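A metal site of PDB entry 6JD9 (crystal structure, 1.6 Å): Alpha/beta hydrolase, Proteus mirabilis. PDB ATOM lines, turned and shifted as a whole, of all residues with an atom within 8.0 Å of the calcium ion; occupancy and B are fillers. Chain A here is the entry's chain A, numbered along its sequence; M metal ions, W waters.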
ATOM      1  N   PHE A 142      25.388 -26.463  21.473  1.00  0.00           N
ATOM      2  CA  PHE A 142      25.698 -26.023  20.135  1.00  0.00           C
ATOM      3  C   PHE A 142      26.781 -26.826  19.446  1.00  0.00           C
ATOM      4  O   PHE A 142      26.665 -27.011  18.206  1.00  0.00           O
ATOM      5  CB  PHE A 142      26.042 -24.518  20.095  1.00  0.00           C
ATOM      6  CG  PHE A 142      24.805 -23.582  20.251  1.00  0.00           C
ATOM      7  CD1 PHE A 142      23.909 -23.479  19.213  1.00  0.00           C
ATOM      8  CD2 PHE A 142      24.645 -22.799  21.362  1.00  0.00           C
ATOM      9  CE1 PHE A 142      22.858 -22.605  19.257  1.00  0.00           C
ATOM     10  CE2 PHE A 142      23.576 -21.940  21.449  1.00  0.00           C
ATOM     11  CZ  PHE A 142      22.708 -21.839  20.395  1.00  0.00           C
ATOM     12  N   GLU A 206       7.158 -23.725  29.597  1.00  0.00           N
ATOM     13  CA  GLU A 206       7.996 -23.193  28.435  1.00  0.00           C
ATOM     14  C   GLU A 206       7.771 -23.841  27.030  1.00  0.00           C
ATOM     15  O   GLU A 206       8.318 -23.324  26.012  1.00  0.00           O
ATOM     16  CB  GLU A 206       9.475 -23.222  28.770  1.00  0.00           C
ATOM     17  CG  GLU A 206       9.945 -22.115  29.703  1.00  0.00           C
ATOM     18  CD  GLU A 206      10.294 -20.813  29.010  1.00  0.00           C
ATOM     19  OE1 GLU A 206      10.502 -20.767  27.752  1.00  0.00           O
ATOM     20  OE2 GLU A 206      10.416 -19.794  29.744  1.00  0.00           O
ATOM     21  N   GLY A 208       8.249 -25.691  23.795  1.00  0.00           N
ATOM     22  CA  GLY A 208       9.427 -26.103  23.069  1.00  0.00           C
ATOM     23  C   GLY A 208      10.739 -26.063  23.734  1.00  0.00           C
ATOM     24  O   GLY A 208      11.571 -26.915  23.588  1.00  0.00           O
ATOM     25  N   ASN A 209      10.895 -25.035  24.616  1.00  0.00           N
ATOM     26  CA  ASN A 209      12.071 -24.922  25.375  1.00  0.00           C
ATOM     27  C   ASN A 209      12.319 -26.038  26.339  1.00  0.00           C
ATOM     28  O   ASN A 209      13.426 -26.225  26.757  1.00  0.00           O
ATOM     29  CB  ASN A 209      12.124 -23.516  26.049  1.00  0.00           C
ATOM     30  CG  ASN A 209      13.066 -22.545  25.357  1.00  0.00           C
ATOM     31  OD1 ASN A 209      13.942 -22.878  24.546  1.00  0.00           O
ATOM     32  ND2 ASN A 209      12.908 -21.322  25.773  1.00  0.00           N
ATOM     33  N   LEU A 210      11.260 -26.846  26.668  1.00  0.00           N
ATOM     34  CA  LEU A 210      11.539 -28.027  27.483  1.00  0.00           C
ATOM     35  C   LEU A 210      12.430 -29.061  26.815  1.00  0.00           C
ATOM     36  O   LEU A 210      13.011 -29.900  27.480  1.00  0.00           O
ATOM     37  CB  LEU A 210      10.222 -28.650  27.880  1.00  0.00           C
ATOM     38  CG  LEU A 210       9.386 -27.785  28.781  1.00  0.00           C
ATOM     39  CD1 LEU A 210       8.058 -28.512  29.044  1.00  0.00           C
ATOM     40  CD2 LEU A 210      10.070 -27.512  30.088  1.00  0.00           C
ATOM     41  N   LEU A 211      12.628 -28.952  25.491  1.00  0.00           N
ATOM     42  CA  LEU A 211      13.516 -29.839  24.749  1.00  0.00           C
ATOM     43  C   LEU A 211      14.895 -29.247  24.408  1.00  0.00           C
ATOM     44  O   LEU A 211      15.771 -29.855  23.785  1.00  0.00           O
ATOM     45  CB  LEU A 211      12.858 -30.241  23.416  1.00  0.00           C
ATOM     46  CG  LEU A 211      11.432 -30.822  23.555  1.00  0.00           C
ATOM     47  CD1 LEU A 211      10.747 -30.972  22.220  1.00  0.00           C
ATOM     48  CD2 LEU A 211      11.607 -32.135  24.248  1.00  0.00           C
ATOM     49  N   ASP A 212      15.131 -28.014  24.935  1.00  0.00           N
ATOM     50  CA  ASP A 212      16.302 -27.272  24.578  1.00  0.00           C
ATOM     51  C   ASP A 212      17.179 -27.137  25.825  1.00  0.00           C
ATOM     52  O   ASP A 212      16.862 -26.325  26.724  1.00  0.00           O
ATOM     53  CB  ASP A 212      15.893 -25.864  24.109  1.00  0.00           C
ATOM     54  CG  ASP A 212      17.118 -25.024  23.684  1.00  0.00           C
ATOM     55  OD1 ASP A 212      18.257 -25.362  23.947  1.00  0.00           O
ATOM     56  OD2 ASP A 212      16.813 -23.943  23.028  1.00  0.00           O
ATOM     57  N   PRO A 213      18.315 -27.855  25.885  1.00  0.00           N
ATOM     58  CA  PRO A 213      19.107 -27.829  27.082  1.00  0.00           C
ATOM     59  C   PRO A 213      19.733 -26.453  27.416  1.00  0.00           C
ATOM     60  O   PRO A 213      20.087 -26.223  28.562  1.00  0.00           O
ATOM     61  CB  PRO A 213      20.267 -28.828  26.807  1.00  0.00           C
ATOM     62  CG  PRO A 213      19.724 -29.666  25.784  1.00  0.00           C
ATOM     63  CD  PRO A 213      18.769 -28.900  24.967  1.00  0.00           C
ATOM     64  N   THR A 214      19.766 -25.551  26.444  1.00  0.00           N
ATOM     65  CA  THR A 214      20.307 -24.277  26.721  1.00  0.00           C
ATOM     66  C   THR A 214      19.377 -23.422  27.593  1.00  0.00           C
ATOM     67  O   THR A 214      19.833 -22.488  28.210  1.00  0.00           O
ATOM     68  CB  THR A 214      20.605 -23.414  25.469  1.00  0.00           C
ATOM     69  OG1 THR A 214      19.415 -23.101  24.768  1.00  0.00           O
ATOM     70  CG2 THR A 214      21.512 -24.127  24.516  1.00  0.00           C
ATOM     71  N   HIS A 215      18.101 -23.707  27.619  1.00  0.00           N
ATOM     72  CA  HIS A 215      17.129 -22.816  28.319  1.00  0.00           C
ATOM     73  C   HIS A 215      17.308 -22.831  29.818  1.00  0.00           C
ATOM     74  O   HIS A 215      17.395 -21.797  30.479  1.00  0.00           O
ATOM     75  CB  HIS A 215      15.726 -23.052  27.868  1.00  0.00           C
ATOM     76  CG  HIS A 215      14.740 -22.150  28.520  1.00  0.00           C
ATOM     77  ND1 HIS A 215      14.838 -20.798  28.376  1.00  0.00           N
ATOM     78  CD2 HIS A 215      13.770 -22.384  29.457  1.00  0.00           C
ATOM     79  CE1 HIS A 215      13.879 -20.239  29.124  1.00  0.00           C
ATOM     80  NE2 HIS A 215      13.272 -21.180  29.813  1.00  0.00           N
ATOM     81  N   ALA A 216      17.453 -24.011  30.374  1.00  0.00           N
ATOM     82  CA  ALA A 216      17.659 -24.095  31.795  1.00  0.00           C
ATOM     83  C   ALA A 216      18.972 -23.506  32.206  1.00  0.00           C
ATOM     84  O   ALA A 216      19.013 -22.868  33.248  1.00  0.00           O
ATOM     85  CB  ALA A 216      17.615 -25.570  32.239  1.00  0.00           C
ATOM     86  N   MET A 218      20.328 -20.841  30.678  1.00  0.00           N
ATOM     87  CA  MET A 218      20.046 -19.396  30.692  1.00  0.00           C
ATOM     88  C   MET A 218      19.338 -19.001  31.970  1.00  0.00           C
ATOM     89  O   MET A 218      19.569 -17.939  32.514  1.00  0.00           O
ATOM     90  CB  MET A 218      19.280 -18.986  29.430  1.00  0.00           C
ATOM     91  CG  MET A 218      20.072 -19.294  28.208  1.00  0.00           C
ATOM     92  SD  MET A 218      21.523 -18.190  28.117  1.00  0.00           S
ATOM     93  CE  MET A 218      20.434 -17.537  27.154  1.00  0.00           C
ATOM     94  N   GLN A 251      11.385 -14.717  26.634  1.00  0.00           N
ATOM     95  CA  GLN A 251      12.376 -15.395  25.797  1.00  0.00           C
ATOM     96  C   GLN A 251      13.748 -15.185  26.384  1.00  0.00           C
ATOM     97  O   GLN A 251      14.050 -14.055  26.856  1.00  0.00           O
ATOM     98  CB  GLN A 251      12.307 -14.940  24.376  1.00  0.00           C
ATOM     99  CG  GLN A 251      10.946 -15.121  23.655  1.00  0.00           C
ATOM    100  CD  GLN A 251      10.510 -16.570  23.500  1.00  0.00           C
ATOM    101  OE1 GLN A 251      11.296 -17.520  23.514  1.00  0.00           O
ATOM    102  NE2 GLN A 251       9.197 -16.715  23.410  1.00  0.00           N
ATOM    103  N   ASP A 252      14.608 -16.184  26.375  1.00  0.00           N
ATOM    104  CA  ASP A 252      15.995 -16.033  26.730  1.00  0.00           C
ATOM    105  C   ASP A 252      16.841 -15.478  25.519  1.00  0.00           C
ATOM    106  O   ASP A 252      16.301 -15.202  24.444  1.00  0.00           O
ATOM    107  CB  ASP A 252      16.578 -17.310  27.322  1.00  0.00           C
ATOM    108  CG  ASP A 252      16.800 -18.399  26.334  1.00  0.00           C
ATOM    109  OD1 ASP A 252      17.252 -18.129  25.200  1.00  0.00           O
ATOM    110  OD2 ASP A 252      16.683 -19.620  26.702  1.00  0.00           O
ATOM    111  N   HIS A 253      18.124 -15.192  25.812  1.00  0.00           N
ATOM    112  CA  HIS A 253      18.962 -14.515  24.831  1.00  0.00           C
ATOM    113  C   HIS A 253      19.014 -15.196  23.515  1.00  0.00           C
ATOM    114  O   HIS A 253      19.010 -14.537  22.494  1.00  0.00           O
ATOM    115  CB  HIS A 253      20.357 -14.424  25.465  1.00  0.00           C
ATOM    116  CG  HIS A 253      21.311 -13.526  24.767  1.00  0.00           C
ATOM    117  ND1 HIS A 253      21.125 -12.172  24.710  1.00  0.00           N
ATOM    118  CD2 HIS A 253      22.482 -13.771  24.123  1.00  0.00           C
ATOM    119  CE1 HIS A 253      22.141 -11.618  24.062  1.00  0.00           C
ATOM    120  NE2 HIS A 253      22.965 -12.570  23.697  1.00  0.00           N
ATOM    121  N   ILE A 254      19.062 -16.522  23.571  1.00  0.00           N
ATOM    122  CA  ILE A 254      19.204 -17.220  22.268  1.00  0.00           C
ATOM    123  C   ILE A 254      17.887 -17.654  21.640  1.00  0.00           C
ATOM    124  O   ILE A 254      17.753 -17.761  20.442  1.00  0.00           O
ATOM    125  CB  ILE A 254      20.169 -18.303  22.288  1.00  0.00           C
ATOM    126  CG1 ILE A 254      19.738 -19.364  23.147  1.00  0.00           C
ATOM    127  CG2 ILE A 254      21.585 -17.856  22.646  1.00  0.00           C
ATOM    128  CD1 ILE A 254      20.485 -20.639  22.958  1.00  0.00           C
ATOM    129  N   ASP A 255      16.845 -17.688  22.454  1.00  0.00           N
ATOM    130  CA  ASP A 255      15.479 -17.811  21.951  1.00  0.00           C
ATOM    131  C   ASP A 255      15.214 -16.704  20.917  1.00  0.00           C
ATOM    132  O   ASP A 255      14.481 -16.827  19.929  1.00  0.00           O
ATOM    133  CB  ASP A 255      14.453 -17.645  23.082  1.00  0.00           C
ATOM    134  CG  ASP A 255      14.261 -18.838  23.948  1.00  0.00           C
ATOM    135  OD1 ASP A 255      14.514 -19.968  23.475  1.00  0.00           O
ATOM    136  OD2 ASP A 255      13.908 -18.644  25.127  1.00  0.00           O
ATOM    137  N   MET A 256      15.748 -15.478  21.170  1.00  0.00           N
ATOM    138  CA  MET A 256      15.491 -14.347  20.315  1.00  0.00           C
ATOM    139  C   MET A 256      16.127 -14.373  18.954  1.00  0.00           C
ATOM    140  O   MET A 256      15.818 -13.572  18.101  1.00  0.00           O
ATOM    141  CB  MET A 256      15.816 -13.000  21.048  1.00  0.00           C
ATOM    142  CG  MET A 256      14.805 -12.686  22.181  1.00  0.00           C
ATOM    143  SD  MET A 256      13.146 -12.471  21.646  1.00  0.00           S
ATOM    144  CE  MET A 256      13.290 -10.870  20.819  1.00  0.00           C
ATOM    145  N   VAL A 257      16.990 -15.360  18.732  1.00  0.00           N
ATOM    146  CA  VAL A 257      17.494 -15.716  17.388  1.00  0.00           C
ATOM    147  C   VAL A 257      17.013 -17.118  17.012  1.00  0.00           C
ATOM    148  O   VAL A 257      17.617 -17.758  16.088  1.00  0.00           O
ATOM    149  CB  VAL A 257      18.999 -15.554  17.229  1.00  0.00           C
ATOM    150  CG1 VAL A 257      19.371 -14.065  17.186  1.00  0.00           C
ATOM    151  CG2 VAL A 257      19.825 -16.269  18.252  1.00  0.00           C
ATOM    152  N   ASN A 258      15.908 -17.533  17.634  1.00  0.00           N
ATOM    153  CA  ASN A 258      15.206 -18.768  17.201  1.00  0.00           C
ATOM    154  C   ASN A 258      16.029 -19.993  17.479  1.00  0.00           C
ATOM    155  O   ASN A 258      15.925 -20.982  16.688  1.00  0.00           O
ATOM    156  CB  ASN A 258      14.693 -18.623  15.780  1.00  0.00           C
ATOM    157  CG  ASN A 258      13.571 -19.622  15.468  1.00  0.00           C
ATOM    158  OD1 ASN A 258      12.764 -19.999  16.354  1.00  0.00           O
ATOM    159  ND2 ASN A 258      13.485 -19.994  14.199  1.00  0.00           N
ATOM    160  N   GLN A 259      16.776 -20.035  18.582  1.00  0.00           N
ATOM    161  CA  GLN A 259      17.701 -21.097  18.926  1.00  0.00           C
ATOM    162  C   GLN A 259      17.270 -21.822  20.227  1.00  0.00           C
ATOM    163  O   GLN A 259      16.675 -21.174  21.129  1.00  0.00           O
ATOM    164  CB  GLN A 259      19.159 -20.597  19.135  1.00  0.00           C
ATOM    165  CG  GLN A 259      19.702 -20.054  17.813  1.00  0.00           C
ATOM    166  CD  GLN A 259      20.159 -21.139  16.850  1.00  0.00           C
ATOM    167  OE1 GLN A 259      19.889 -22.311  17.026  1.00  0.00           O
ATOM    168  NE2 GLN A 259      20.803 -20.729  15.788  1.00  0.00           N
ATOM    169  N   VAL A 260      17.579 -23.114  20.357  1.00  0.00           N
ATOM    170  CA  VAL A 260      18.380 -23.894  19.415  1.00  0.00           C
ATOM    171  C   VAL A 260      17.466 -24.487  18.374  1.00  0.00           C
ATOM    172  O   VAL A 260      16.468 -25.188  18.705  1.00  0.00           O
ATOM    173  CB  VAL A 260      19.164 -25.001  20.159  1.00  0.00           C
ATOM    174  CG1 VAL A 260      19.911 -25.903  19.199  1.00  0.00           C
ATOM    175  CG2 VAL A 260      20.091 -24.459  21.173  1.00  0.00           C
ATOM    176  N   ALA A 261      17.741 -24.261  17.109  1.00  0.00           N
ATOM    177  CA  ALA A 261      16.979 -24.894  16.011  1.00  0.00           C
ATOM    178  C   ALA A 261      15.470 -24.777  16.154  1.00  0.00           C
ATOM    179  O   ALA A 261      14.740 -25.803  15.973  1.00  0.00           O
ATOM    180  CB  ALA A 261      17.492 -26.356  15.878  1.00  0.00           C
ATOM    181  N   GLY A 262      14.928 -23.603  16.491  1.00  0.00           N
ATOM    182  CA  GLY A 262      13.560 -23.348  16.596  1.00  0.00           C
ATOM    183  C   GLY A 262      12.883 -23.752  17.846  1.00  0.00           C
ATOM    184  O   GLY A 262      11.668 -23.547  17.915  1.00  0.00           O
ATOM    185  N   LEU A 263      13.635 -24.166  18.845  1.00  0.00           N
ATOM    186  CA  LEU A 263      13.094 -24.489  20.175  1.00  0.00           C
ATOM    187  C   LEU A 263      13.103 -23.173  21.017  1.00  0.00           C
ATOM    188  O   LEU A 263      14.197 -22.792  21.460  1.00  0.00           O
ATOM    189  CB  LEU A 263      13.844 -25.606  20.892  1.00  0.00           C
ATOM    190  CG  LEU A 263      13.906 -26.990  20.125  1.00  0.00           C
ATOM    191  CD1 LEU A 263      14.868 -27.908  20.740  1.00  0.00           C
ATOM    192  CD2 LEU A 263      12.483 -27.552  20.045  1.00  0.00           C
ATOM    193  N   VAL A 264      11.922 -22.607  21.193  1.00  0.00           N
ATOM    194  CA  VAL A 264      11.782 -21.308  21.847  1.00  0.00           C
ATOM    195  C   VAL A 264      10.698 -21.358  22.883  1.00  0.00           C
ATOM    196  O   VAL A 264      10.087 -22.441  23.093  1.00  0.00           O
ATOM    197  CB  VAL A 264      11.574 -20.250  20.819  1.00  0.00           C
ATOM    198  CG1 VAL A 264      12.712 -20.161  19.767  1.00  0.00           C
ATOM    199  CG2 VAL A 264      10.256 -20.392  20.083  1.00  0.00           C
ATOM    200  N   GLY A 265      10.470 -20.273  23.579  1.00  0.00           N
ATOM    201  CA  GLY A 265       9.448 -20.317  24.639  1.00  0.00           C
ATOM    202  C   GLY A 265       8.039 -20.128  24.111  1.00  0.00           C
ATOM    203  O   GLY A 265       7.738 -19.340  23.243  1.00  0.00           O
HETATM  204 CA    CA M   1      15.535 -21.978  23.079  1.00  0.00          CA
HETATM  205  O   HOH W   1      17.042 -21.424  24.830  1.00  0.00           O
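The backbone NH (N) of Asp 255 is in hydrogen-bond range of the side-chain carboxylate (OD1) of Asp 252, at 2.8 Å.
OD2 of Asp 255 lies close to OE1 of Gln 251, at 3.3 Å.
The side-chain carboxylate (OD2) of Asp 212 lies close to the backbone NH (N) of Val 260 (2.9 Å).
The side-chain hydroxyl (OG1) of Thr 214 sits at hydrogen-bond distance from the side-chain carboxylate (OD1) of Asp 212 (2.7 Å).
The backbone carbonyl oxygen (O) of Val 264 lies within hydrogen-bond range of the backbone NH (N) of Asn 209, at 3.1 Å.
A ring nitrogen (ND1) of His 215 sits at hydrogen-bond distance from the side-chain amide nitrogen (ND2) of Asn 209 (3.3 Å).
ND2 of Asn 209 sits at hydrogen-bond distance from OE1 of Glu 206.
OE1 of Gln 259 sits at hydrogen-bond distance from N of Ala 261.
Val 260 touches the calcium ion.
Six residues have an atom within 4 Å of the calcium ion: Asn 209, Asp 212, Asp 255, Gln 259, Val 260 and Leu 263.
The nearest printed residue that does not touch the calcium ion is Val 264 (4.01 Å).
The calcium ion is bound by O of Leu 263 (2.3 Å), OD1 of Asp 255 (2.3 Å), OD2 of Asp 212 (2.3 Å), OD1 of Asn 209 (2.3 Å), water W1 (2.4 Å) and O of Gln 259 (2.4 Å).
The calcium ion has six donor atoms within binding distance.
Water W1 lies within hydrogen-bond range of the side-chain carboxylate of Asp 252 (2.6 Å) and the side-chain hydroxyl of Thr 214 (2.9 Å).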
